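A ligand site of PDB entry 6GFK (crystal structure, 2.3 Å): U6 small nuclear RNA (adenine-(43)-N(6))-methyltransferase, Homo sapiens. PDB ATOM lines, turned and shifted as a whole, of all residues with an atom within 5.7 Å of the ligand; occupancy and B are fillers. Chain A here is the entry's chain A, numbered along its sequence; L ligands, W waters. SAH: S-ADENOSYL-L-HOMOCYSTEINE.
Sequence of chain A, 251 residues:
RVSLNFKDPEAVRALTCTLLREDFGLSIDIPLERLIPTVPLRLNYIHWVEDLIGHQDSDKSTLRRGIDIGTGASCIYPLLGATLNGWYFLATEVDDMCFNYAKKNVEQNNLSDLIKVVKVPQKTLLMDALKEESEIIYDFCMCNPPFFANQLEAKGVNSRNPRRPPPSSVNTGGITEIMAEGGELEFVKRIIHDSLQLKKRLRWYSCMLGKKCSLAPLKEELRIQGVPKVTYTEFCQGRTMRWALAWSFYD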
ATOM      1  N   LEU A  35      24.342  23.394  -0.066  1.00  0.00           N
ATOM      2  CA  LEU A  35      25.183  24.329   0.708  1.00  0.00           C
ATOM      3  C   LEU A  35      24.442  25.630   1.019  1.00  0.00           C
ATOM      4  O   LEU A  35      23.866  26.240   0.121  1.00  0.00           O
ATOM      5  CB  LEU A  35      26.498  24.613  -0.077  1.00  0.00           C
ATOM      6  CG  LEU A  35      27.374  25.789   0.404  1.00  0.00           C
ATOM      7  CD1 LEU A  35      28.026  25.479   1.768  1.00  0.00           C
ATOM      8  CD2 LEU A  35      28.428  26.122  -0.636  1.00  0.00           C
ATOM      9  N   ILE A  36      24.426  26.013   2.309  1.00  0.00           N
ATOM     10  CA  ILE A  36      23.804  27.232   2.810  1.00  0.00           C
ATOM     11  C   ILE A  36      24.896  28.297   2.817  1.00  0.00           C
ATOM     12  O   ILE A  36      25.864  28.134   3.563  1.00  0.00           O
ATOM     13  CB  ILE A  36      23.155  27.076   4.229  1.00  0.00           C
ATOM     14  CG1 ILE A  36      22.267  25.778   4.370  1.00  0.00           C
ATOM     15  CG2 ILE A  36      22.394  28.336   4.645  1.00  0.00           C
ATOM     16  CD1 ILE A  36      20.972  25.661   3.408  1.00  0.00           C
ATOM     17  N   PRO A  37      24.802  29.363   1.985  1.00  0.00           N
ATOM     18  CA  PRO A  37      25.846  30.396   1.993  1.00  0.00           C
ATOM     19  C   PRO A  37      25.807  31.252   3.259  1.00  0.00           C
ATOM     20  O   PRO A  37      24.738  31.457   3.819  1.00  0.00           O
ATOM     21  CB  PRO A  37      25.531  31.229   0.759  1.00  0.00           C
ATOM     22  CG  PRO A  37      24.084  31.081   0.575  1.00  0.00           C
ATOM     23  CD  PRO A  37      23.724  29.713   1.025  1.00  0.00           C
ATOM     24  N   ARG A  42      30.605  35.759   1.561  1.00  0.00           N
ATOM     25  CA  ARG A  42      30.216  35.971   0.185  1.00  0.00           C
ATOM     26  C   ARG A  42      30.464  37.448  -0.192  1.00  0.00           C
ATOM     27  O   ARG A  42      30.985  37.721  -1.266  1.00  0.00           O
ATOM     28  CB  ARG A  42      28.755  35.568  -0.044  1.00  0.00           C
ATOM     29  CG  ARG A  42      28.412  34.088   0.207  1.00  0.00           C
ATOM     30  CD  ARG A  42      29.422  33.155  -0.411  1.00  0.00           C
ATOM     31  NE  ARG A  42      29.004  31.766  -0.466  1.00  0.00           N
ATOM     32  CZ  ARG A  42      29.230  30.884   0.499  1.00  0.00           C
ATOM     33  NH1 ARG A  42      28.868  29.619   0.351  1.00  0.00           N
ATOM     34  NH2 ARG A  42      29.819  31.261   1.621  1.00  0.00           N
ATOM     35  N   ASP A  68      29.823  33.370 -12.806  1.00  0.00           N
ATOM     36  CA  ASP A  68      29.871  32.647 -11.529  1.00  0.00           C
ATOM     37  C   ASP A  68      29.799  31.169 -11.829  1.00  0.00           C
ATOM     38  O   ASP A  68      28.767  30.705 -12.306  1.00  0.00           O
ATOM     39  CB  ASP A  68      28.749  33.089 -10.585  1.00  0.00           C
ATOM     40  CG  ASP A  68      28.744  32.421  -9.222  1.00  0.00           C
ATOM     41  OD1 ASP A  68      29.829  31.945  -8.776  1.00  0.00           O
ATOM     42  OD2 ASP A  68      27.678  32.390  -8.582  1.00  0.00           O
ATOM     43  N   ILE A  69      30.917  30.448 -11.662  1.00  0.00           N
ATOM     44  CA  ILE A  69      30.994  29.004 -11.910  1.00  0.00           C
ATOM     45  C   ILE A  69      30.437  28.267 -10.697  1.00  0.00           C
ATOM     46  O   ILE A  69      31.051  28.339  -9.629  1.00  0.00           O
ATOM     47  CB  ILE A  69      32.448  28.522 -12.250  1.00  0.00           C
ATOM     48  CG1 ILE A  69      33.085  29.363 -13.388  1.00  0.00           C
ATOM     49  CG2 ILE A  69      32.474  26.998 -12.580  1.00  0.00           C
ATOM     50  CD1 ILE A  69      34.657  29.344 -13.389  1.00  0.00           C
ATOM     51  N   GLY A  70      29.293  27.614 -10.847  1.00  0.00           N
ATOM     52  CA  GLY A  70      28.659  26.877  -9.746  1.00  0.00           C
ATOM     53  C   GLY A  70      27.944  27.799  -8.797  1.00  0.00           C
ATOM     54  O   GLY A  70      28.319  27.936  -7.642  1.00  0.00           O
ATOM     55  N   THR A  71      26.914  28.452  -9.301  1.00  0.00           N
ATOM     56  CA  THR A  71      26.174  29.497  -8.596  1.00  0.00           C
ATOM     57  C   THR A  71      25.412  29.001  -7.343  1.00  0.00           C
ATOM     58  O   THR A  71      25.130  29.807  -6.461  1.00  0.00           O
ATOM     59  CB  THR A  71      25.285  30.246  -9.600  1.00  0.00           C
ATOM     60  OG1 THR A  71      25.098  31.587  -9.148  1.00  0.00           O
ATOM     61  CG2 THR A  71      23.950  29.549  -9.908  1.00  0.00           C
ATOM     62  N   GLY A  72      25.126  27.692  -7.252  1.00  0.00           N
ATOM     63  CA  GLY A  72      24.399  27.081  -6.152  1.00  0.00           C
ATOM     64  C   GLY A  72      22.911  27.372  -6.203  1.00  0.00           C
ATOM     65  O   GLY A  72      22.451  28.065  -7.112  1.00  0.00           O
ATOM     66  N   ALA A  73      22.147  26.838  -5.245  1.00  0.00           N
ATOM     67  CA  ALA A  73      20.689  27.051  -5.166  1.00  0.00           C
ATOM     68  C   ALA A  73      20.360  28.503  -4.799  1.00  0.00           C
ATOM     69  O   ALA A  73      19.318  29.011  -5.196  1.00  0.00           O
ATOM     70  CB  ALA A  73      20.080  26.118  -4.116  1.00  0.00           C
ATOM     71  N   SER A  74      21.235  29.156  -4.037  1.00  0.00           N
ATOM     72  CA  SER A  74      21.075  30.533  -3.582  1.00  0.00           C
ATOM     73  C   SER A  74      21.319  31.550  -4.682  1.00  0.00           C
ATOM     74  O   SER A  74      20.727  32.627  -4.621  1.00  0.00           O
ATOM     75  CB  SER A  74      22.037  30.820  -2.438  1.00  0.00           C
ATOM     76  OG  SER A  74      23.372  30.646  -2.883  1.00  0.00           O
ATOM     77  N   ILE A  76      23.931  33.244  -4.860  1.00  0.00           N
ATOM     78  CA  ILE A  76      24.348  34.273  -3.935  1.00  0.00           C
ATOM     79  C   ILE A  76      25.297  35.315  -4.533  1.00  0.00           C
ATOM     80  O   ILE A  76      25.074  36.512  -4.291  1.00  0.00           O
ATOM     81  CB  ILE A  76      24.879  33.682  -2.587  1.00  0.00           C
ATOM     82  CG1 ILE A  76      25.043  34.776  -1.491  1.00  0.00           C
ATOM     83  CG2 ILE A  76      26.153  32.841  -2.755  1.00  0.00           C
ATOM     84  CD1 ILE A  76      23.767  35.463  -1.064  1.00  0.00           C
ATOM     85  N   TYR A  77      26.352  34.905  -5.274  1.00  0.00           N
ATOM     86  CA  TYR A  77      27.285  35.865  -5.868  1.00  0.00           C
ATOM     87  C   TYR A  77      26.570  36.760  -6.876  1.00  0.00           C
ATOM     88  O   TYR A  77      26.621  37.986  -6.703  1.00  0.00           O
ATOM     89  CB  TYR A  77      28.537  35.192  -6.456  1.00  0.00           C
ATOM     90  CG  TYR A  77      29.438  34.501  -5.459  1.00  0.00           C
ATOM     91  CD1 TYR A  77      29.841  35.144  -4.292  1.00  0.00           C
ATOM     92  CD2 TYR A  77      29.966  33.238  -5.725  1.00  0.00           C
ATOM     93  CE1 TYR A  77      30.722  34.526  -3.391  1.00  0.00           C
ATOM     94  CE2 TYR A  77      30.806  32.594  -4.819  1.00  0.00           C
ATOM     95  CZ  TYR A  77      31.181  33.240  -3.662  1.00  0.00           C
ATOM     96  OH  TYR A  77      32.033  32.585  -2.800  1.00  0.00           O
ATOM     97  N   THR A  92      26.487  29.715 -13.884  1.00  0.00           N
ATOM     98  CA  THR A  92      26.428  28.316 -14.335  1.00  0.00           C
ATOM     99  C   THR A  92      26.172  27.339 -13.208  1.00  0.00           C
ATOM    100  O   THR A  92      26.526  27.579 -12.054  1.00  0.00           O
ATOM    101  CB  THR A  92      27.679  27.925 -15.155  1.00  0.00           C
ATOM    102  OG1 THR A  92      28.805  27.849 -14.307  1.00  0.00           O
ATOM    103  CG2 THR A  92      27.966  28.904 -16.304  1.00  0.00           C
ATOM    104  N   GLU A  93      25.555  26.205 -13.578  1.00  0.00           N
ATOM    105  CA  GLU A  93      25.257  25.088 -12.707  1.00  0.00           C
ATOM    106  C   GLU A  93      25.172  23.784 -13.448  1.00  0.00           C
ATOM    107  O   GLU A  93      24.615  23.733 -14.536  1.00  0.00           O
ATOM    108  CB  GLU A  93      23.925  25.294 -11.959  1.00  0.00           C
ATOM    109  CG  GLU A  93      24.070  25.495 -10.462  1.00  0.00           C
ATOM    110  CD  GLU A  93      25.056  24.645  -9.694  1.00  0.00           C
ATOM    111  OE1 GLU A  93      25.625  25.163  -8.718  1.00  0.00           O
ATOM    112  OE2 GLU A  93      25.259  23.451 -10.044  1.00  0.00           O
ATOM    113  N   VAL A  94      25.667  22.702 -12.821  1.00  0.00           N
ATOM    114  CA  VAL A  94      25.562  21.340 -13.346  1.00  0.00           C
ATOM    115  C   VAL A  94      24.459  20.596 -12.594  1.00  0.00           C
ATOM    116  O   VAL A  94      23.864  19.669 -13.149  1.00  0.00           O
ATOM    117  CB  VAL A  94      26.895  20.523 -13.386  1.00  0.00           C
ATOM    118  CG1 VAL A  94      27.911  21.179 -14.312  1.00  0.00           C
ATOM    119  CG2 VAL A  94      27.496  20.313 -12.002  1.00  0.00           C
ATOM    120  N   ASP A  95      24.196  20.991 -11.327  1.00  0.00           N
ATOM    121  CA  ASP A  95      23.193  20.324 -10.470  1.00  0.00           C
ATOM    122  C   ASP A  95      21.788  20.832 -10.782  1.00  0.00           C
ATOM    123  O   ASP A  95      21.561  22.032 -10.757  1.00  0.00           O
ATOM    124  CB  ASP A  95      23.532  20.502  -8.994  1.00  0.00           C
ATOM    125  CG  ASP A  95      22.652  19.717  -8.057  1.00  0.00           C
ATOM    126  OD1 ASP A  95      22.792  18.472  -8.006  1.00  0.00           O
ATOM    127  OD2 ASP A  95      21.828  20.345  -7.364  1.00  0.00           O
ATOM    128  N   CYS A  98      20.013  22.797  -7.785  1.00  0.00           N
ATOM    129  CA  CYS A  98      20.669  24.094  -7.691  1.00  0.00           C
ATOM    130  C   CYS A  98      20.218  25.022  -8.825  1.00  0.00           C
ATOM    131  O   CYS A  98      19.953  26.193  -8.578  1.00  0.00           O
ATOM    132  CB  CYS A  98      22.187  23.937  -7.691  1.00  0.00           C
ATOM    133  SG  CYS A  98      22.888  23.413  -6.121  1.00  0.00           S
ATOM    134  N   VAL A 120      24.697  23.719 -17.434  1.00  0.00           N
ATOM    135  CA  VAL A 120      25.805  23.305 -18.309  1.00  0.00           C
ATOM    136  C   VAL A 120      26.139  21.801 -18.151  1.00  0.00           C
ATOM    137  O   VAL A 120      25.891  21.258 -17.062  1.00  0.00           O
ATOM    138  CB  VAL A 120      27.078  24.210 -18.114  1.00  0.00           C
ATOM    139  CG1 VAL A 120      26.782  25.668 -18.437  1.00  0.00           C
ATOM    140  CG2 VAL A 120      27.665  24.075 -16.703  1.00  0.00           C
ATOM    141  N   PRO A 121      26.703  21.105 -19.180  1.00  0.00           N
ATOM    142  CA  PRO A 121      27.071  19.692 -18.995  1.00  0.00           C
ATOM    143  C   PRO A 121      28.187  19.537 -17.959  1.00  0.00           C
ATOM    144  O   PRO A 121      29.032  20.430 -17.835  1.00  0.00           O
ATOM    145  CB  PRO A 121      27.520  19.244 -20.402  1.00  0.00           C
ATOM    146  CG  PRO A 121      27.043  20.329 -21.343  1.00  0.00           C
ATOM    147  CD  PRO A 121      27.055  21.583 -20.543  1.00  0.00           C
ATOM    148  N   GLN A 122      28.176  18.422 -17.200  1.00  0.00           N
ATOM    149  CA  GLN A 122      29.114  18.104 -16.112  1.00  0.00           C
ATOM    150  C   GLN A 122      30.611  18.186 -16.496  1.00  0.00           C
ATOM    151  O   GLN A 122      31.424  18.673 -15.705  1.00  0.00           O
ATOM    152  CB  GLN A 122      28.781  16.740 -15.463  1.00  0.00           C
ATOM    153  CG  GLN A 122      28.918  15.490 -16.367  1.00  0.00           C
ATOM    154  CD  GLN A 122      27.709  15.142 -17.219  1.00  0.00           C
ATOM    155  OE1 GLN A 122      26.931  15.993 -17.663  1.00  0.00           O
ATOM    156  NE2 GLN A 122      27.551  13.849 -17.503  1.00  0.00           N
ATOM    157  N   LYS A 123      30.951  17.761 -17.720  1.00  0.00           N
ATOM    158  CA  LYS A 123      32.326  17.781 -18.225  1.00  0.00           C
ATOM    159  C   LYS A 123      32.833  19.201 -18.598  1.00  0.00           C
ATOM    160  O   LYS A 123      34.028  19.373 -18.843  1.00  0.00           O
ATOM    161  CB  LYS A 123      32.438  16.843 -19.435  1.00  0.00           C
ATOM    162  N   THR A 124      31.927  20.203 -18.635  1.00  0.00           N
ATOM    163  CA  THR A 124      32.249  21.569 -19.051  1.00  0.00           C
ATOM    164  C   THR A 124      32.559  22.529 -17.884  1.00  0.00           C
ATOM    165  O   THR A 124      32.210  22.251 -16.735  1.00  0.00           O
ATOM    166  CB  THR A 124      31.155  22.131 -19.997  1.00  0.00           C
ATOM    167  OG1 THR A 124      30.002  22.523 -19.248  1.00  0.00           O
ATOM    168  CG2 THR A 124      30.777  21.173 -21.115  1.00  0.00           C
ATOM    169  N   LEU A 125      33.203  23.658 -18.200  1.00  0.00           N
ATOM    170  CA  LEU A 125      33.559  24.683 -17.231  1.00  0.00           C
ATOM    171  C   LEU A 125      33.401  26.106 -17.829  1.00  0.00           C
ATOM    172  O   LEU A 125      32.273  26.572 -17.917  1.00  0.00           O
ATOM    173  CB  LEU A 125      34.957  24.414 -16.692  1.00  0.00           C
ATOM    174  CG  LEU A 125      35.314  24.975 -15.327  1.00  0.00           C
ATOM    175  CD1 LEU A 125      34.664  24.178 -14.232  1.00  0.00           C
ATOM    176  CD2 LEU A 125      36.769  24.869 -15.112  1.00  0.00           C
ATOM    177  N   ASN A 144      33.202  29.434  -6.068  1.00  0.00           N
ATOM    178  CA  ASN A 144      33.264  28.782  -4.753  1.00  0.00           C
ATOM    179  C   ASN A 144      33.200  27.320  -5.176  1.00  0.00           C
ATOM    180  O   ASN A 144      32.143  26.844  -5.602  1.00  0.00           O
ATOM    181  CB  ASN A 144      32.125  29.148  -3.814  1.00  0.00           C
ATOM    182  CG  ASN A 144      32.327  28.564  -2.435  1.00  0.00           C
ATOM    183  OD1 ASN A 144      33.374  27.974  -2.131  1.00  0.00           O
ATOM    184  ND2 ASN A 144      31.339  28.691  -1.573  1.00  0.00           N
ATOM    185  N   PRO A 145      34.357  26.652  -5.289  1.00  0.00           N
ATOM    186  CA  PRO A 145      34.379  25.321  -5.923  1.00  0.00           C
ATOM    187  C   PRO A 145      33.724  24.167  -5.162  1.00  0.00           C
ATOM    188  O   PRO A 145      33.704  24.168  -3.931  1.00  0.00           O
ATOM    189  CB  PRO A 145      35.878  25.057  -6.121  1.00  0.00           C
ATOM    190  CG  PRO A 145      36.541  25.861  -5.053  1.00  0.00           C
ATOM    191  CD  PRO A 145      35.718  27.091  -4.904  1.00  0.00           C
ATOM    192  N   PRO A 146      33.235  23.136  -5.895  1.00  0.00           N
ATOM    193  CA  PRO A 146      32.680  21.954  -5.212  1.00  0.00           C
ATOM    194  C   PRO A 146      33.786  21.088  -4.587  1.00  0.00           C
ATOM    195  O   PRO A 146      34.956  21.216  -4.936  1.00  0.00           O
ATOM    196  CB  PRO A 146      31.946  21.214  -6.336  1.00  0.00           C
ATOM    197  CG  PRO A 146      32.744  21.545  -7.543  1.00  0.00           C
ATOM    198  CD  PRO A 146      33.200  22.967  -7.367  1.00  0.00           C
ATOM    199  N   PHE A 148      34.608  17.440  -4.591  1.00  0.00           N
ATOM    200  CA  PHE A 148      34.393  16.128  -5.207  1.00  0.00           C
ATOM    201  C   PHE A 148      35.513  15.197  -4.797  1.00  0.00           C
ATOM    202  O   PHE A 148      36.688  15.566  -4.869  1.00  0.00           O
ATOM    203  CB  PHE A 148      34.375  16.219  -6.753  1.00  0.00           C
ATOM    204  CG  PHE A 148      33.235  16.968  -7.389  1.00  0.00           C
ATOM    205  CD1 PHE A 148      31.918  16.743  -6.989  1.00  0.00           C
ATOM    206  CD2 PHE A 148      33.470  17.858  -8.432  1.00  0.00           C
ATOM    207  CE1 PHE A 148      30.860  17.427  -7.605  1.00  0.00           C
ATOM    208  CE2 PHE A 148      32.399  18.524  -9.049  1.00  0.00           C
ATOM    209  CZ  PHE A 148      31.113  18.325  -8.618  1.00  0.00           C
ATOM    210  N   PHE A 187      39.972  20.882  -9.244  1.00  0.00           N
ATOM    211  CA  PHE A 187      38.926  21.736  -9.803  1.00  0.00           C
ATOM    212  C   PHE A 187      39.498  23.096 -10.228  1.00  0.00           C
ATOM    213  O   PHE A 187      39.129  23.586 -11.288  1.00  0.00           O
ATOM    214  CB  PHE A 187      37.744  21.897  -8.850  1.00  0.00           C
ATOM    215  CG  PHE A 187      36.532  22.507  -9.523  1.00  0.00           C
ATOM    216  CD1 PHE A 187      36.369  23.884  -9.569  1.00  0.00           C
ATOM    217  CD2 PHE A 187      35.586  21.705 -10.160  1.00  0.00           C
ATOM    218  CE1 PHE A 187      35.271  24.455 -10.216  1.00  0.00           C
ATOM    219  CE2 PHE A 187      34.495  22.283 -10.803  1.00  0.00           C
ATOM    220  CZ  PHE A 187      34.322  23.654 -10.804  1.00  0.00           C
ATOM    221  N   ARG A 190      41.492  22.995 -13.393  1.00  0.00           N
ATOM    222  CA  ARG A 190      40.595  23.008 -14.559  1.00  0.00           C
ATOM    223  C   ARG A 190      40.286  24.446 -14.968  1.00  0.00           C
ATOM    224  O   ARG A 190      40.226  24.724 -16.166  1.00  0.00           O
ATOM    225  CB  ARG A 190      39.288  22.250 -14.274  1.00  0.00           C
ATOM    226  CG  ARG A 190      39.411  20.730 -14.305  1.00  0.00           C
ATOM    227  CD  ARG A 190      38.125  20.068 -13.830  1.00  0.00           C
ATOM    228  NE  ARG A 190      37.009  20.224 -14.780  1.00  0.00           N
ATOM    229  CZ  ARG A 190      35.724  20.047 -14.468  1.00  0.00           C
ATOM    230  NH1 ARG A 190      35.373  19.695 -13.237  1.00  0.00           N
ATOM    231  NH2 ARG A 190      34.783  20.215 -15.392  1.00  0.00           N
HETATM  232  N   SAH L   1      28.500  29.600  -5.294  1.00  0.00           N
HETATM  233  CA  SAH L   1      27.675  28.878  -4.299  1.00  0.00           C
HETATM  234  CB  SAH L   1      27.734  27.295  -4.376  1.00  0.00           C
HETATM  235  CG  SAH L   1      29.164  26.786  -4.295  1.00  0.00           C
HETATM  236  SD  SAH L   1      29.194  24.973  -4.168  1.00  0.00           S
HETATM  237  C   SAH L   1      28.100  29.437  -2.896  1.00  0.00           C
HETATM  238  O   SAH L   1      27.308  29.081  -1.925  1.00  0.00           O
HETATM  239  OXT SAH L   1      29.092  30.121  -2.731  1.00  0.00           O
HETATM  240  C5' SAH L   1      29.862  24.463  -5.771  1.00  0.00           C
HETATM  241  C4' SAH L   1      28.773  24.347  -6.824  1.00  0.00           C
HETATM  242  O4' SAH L   1      29.372  24.177  -8.118  1.00  0.00           O
HETATM  243  C3' SAH L   1      27.751  23.208  -6.649  1.00  0.00           C
HETATM  244  O3' SAH L   1      26.444  23.767  -6.617  1.00  0.00           O
HETATM  245  C2' SAH L   1      27.967  22.324  -7.880  1.00  0.00           C
HETATM  246  O2' SAH L   1      26.776  21.716  -8.377  1.00  0.00           O
HETATM  247  C1' SAH L   1      28.524  23.341  -8.886  1.00  0.00           C
HETATM  248  N9  SAH L   1      29.298  22.786 -10.004  1.00  0.00           N
HETATM  249  C8  SAH L   1      30.140  21.703  -9.988  1.00  0.00           C
HETATM  250  N7  SAH L   1      30.784  21.510 -11.115  1.00  0.00           N
HETATM  251  C5  SAH L   1      30.336  22.535 -11.927  1.00  0.00           C
HETATM  252  C6  SAH L   1      30.656  22.924 -13.255  1.00  0.00           C
HETATM  253  N6  SAH L   1      31.544  22.282 -14.016  1.00  0.00           N
HETATM  254  N1  SAH L   1      30.025  23.998 -13.770  1.00  0.00           N
HETATM  255  C2  SAH L   1      29.124  24.644 -13.018  1.00  0.00           C
HETATM  256  N3  SAH L   1      28.758  24.384 -11.760  1.00  0.00           N
HETATM  257  C4  SAH L   1      29.404  23.323 -11.260  1.00  0.00           C
HETATM  258  O   HOH W   1      26.877  31.773  -6.013  1.00  0.00           O
HETATM  259  O   HOH W   2      30.588  26.070 -15.686  1.00  0.00           O
HETATM  260  O   HOH W   3      31.979  19.057 -12.641  1.00  0.00           O
HETATM  261  O   HOH W   4      24.756  28.381  -2.297  1.00  0.00           O
HETATM  262  O   HOH W   5      30.487  29.825  -7.233  1.00  0.00           O
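N3 of the ligand sits close to N of Gly 70, at 3.4 Å. The backbone carbonyl oxygen (O) of Gly 70 lies within hydrogen-bond range of a nitrogen (N) of the ligand (2.9 Å). An oxygen (OXT) of the ligand is in hydrogen-bond range of the side-chain amide nitrogen (ND2) of Asn 144 (2.9 Å). NE of Arg 42 is in salt-bridge range of OXT of the ligand (2.8 Å). O of Thr 124 lies within hydrogen-bond range of N6 of the ligand (2.8 Å). The side-chain carboxylate of Glu 93 is in hydrogen-bond range of an oxygen (O3') of the ligand, 2.7 Å away. SG of Cys 98 is in hydrogen-bond range of O3' of the ligand, at 3.6 Å.
The side-chain hydroxyl (OG1) of Thr 71 sits at hydrogen-bond distance from the side-chain carboxylate (OD2) of Asp 68, at 2.8 Å. O of Thr 92 lies within hydrogen-bond range of N of Thr 71 (2.9 Å). OG1 of Thr 124 lies within hydrogen-bond range of O of Pro 121 (2.7 Å). The backbone NH (N) of Gly 70 sits at hydrogen-bond distance from the backbone carbonyl oxygen (O) of Thr 92, at 3.0 Å. The backbone NH (N) of Ile 76 lies close to the side-chain hydroxyl (OG) of Ser 74 (3.3 Å). OE2 of Glu 93 lies within hydrogen-bond range of N of Asp 95, at 3.0 Å. The backbone carbonyl oxygen (O) of Glu 93 sits at hydrogen-bond distance from the backbone NH (N) of Val 120. OD2 of Asp 95 sits at hydrogen-bond distance from N of Cys 98 (3.1 Å).
Leu 35 touches the ligand. Pro 37 touches the ligand (CB to O, 3.9 Å). Thr 71 touches the ligand. Gly 72 touches the ligand. Ile 76 touches the ligand. Tyr 77 touches the ligand. Thr 92 touches the ligand. Val 94 touches the ligand. Asp 95 touches the ligand (CB to O2', 3.5 Å). Val 120 touches the ligand (CG2 to N1, 3.8 Å). Gln 122 touches the ligand. Leu 125 touches the ligand. Pro 145 touches the ligand (C to C5', 3.9 Å). Pro 146 touches the ligand (CG to C8, 3.6 Å). Phe 148 touches the ligand (CZ to C8, 3.8 Å). Phe 187 touches the ligand (CE2 to N7, 3.8 Å). Hydrophobic or aromatic side chains that line the ligand: Leu 35, Pro 37, Ile 76, Tyr 77, Val 94, Val 120, Leu 125, Pro 146, Phe 148 and Phe 187. Along chain A the residues within 4 Å of the ligand span positions 35 to 187. The nearest printed residue that does not touch the ligand is Ile 69 (4.1 Å).
Water W4 lies within hydrogen-bond range of an oxygen (O) of the ligand (2.7 Å), the side-chain hydroxyl of Ser 74 (2.7 Å) and the backbone carbonyl oxygen of Leu 35 (3.4 Å). Water W1 lies within hydrogen-bond range of the backbone carbonyl oxygen of Thr 71, the side-chain carboxylate of Asp 68, a nitrogen (N) of the ligand, the backbone NH of Tyr 77 and the backbone NH of Ile 76. Water W2 lies within hydrogen-bond range of the backbone carbonyl oxygen of Leu 125 (2.8 Å), the side-chain hydroxyl of Thr 92 (2.9 Å) and a nitrogen (N1) of the ligand (2.9 Å). Water W3 bridges N7 of the ligand (3.1 Å) and O of Gln 122 (3.1 Å).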
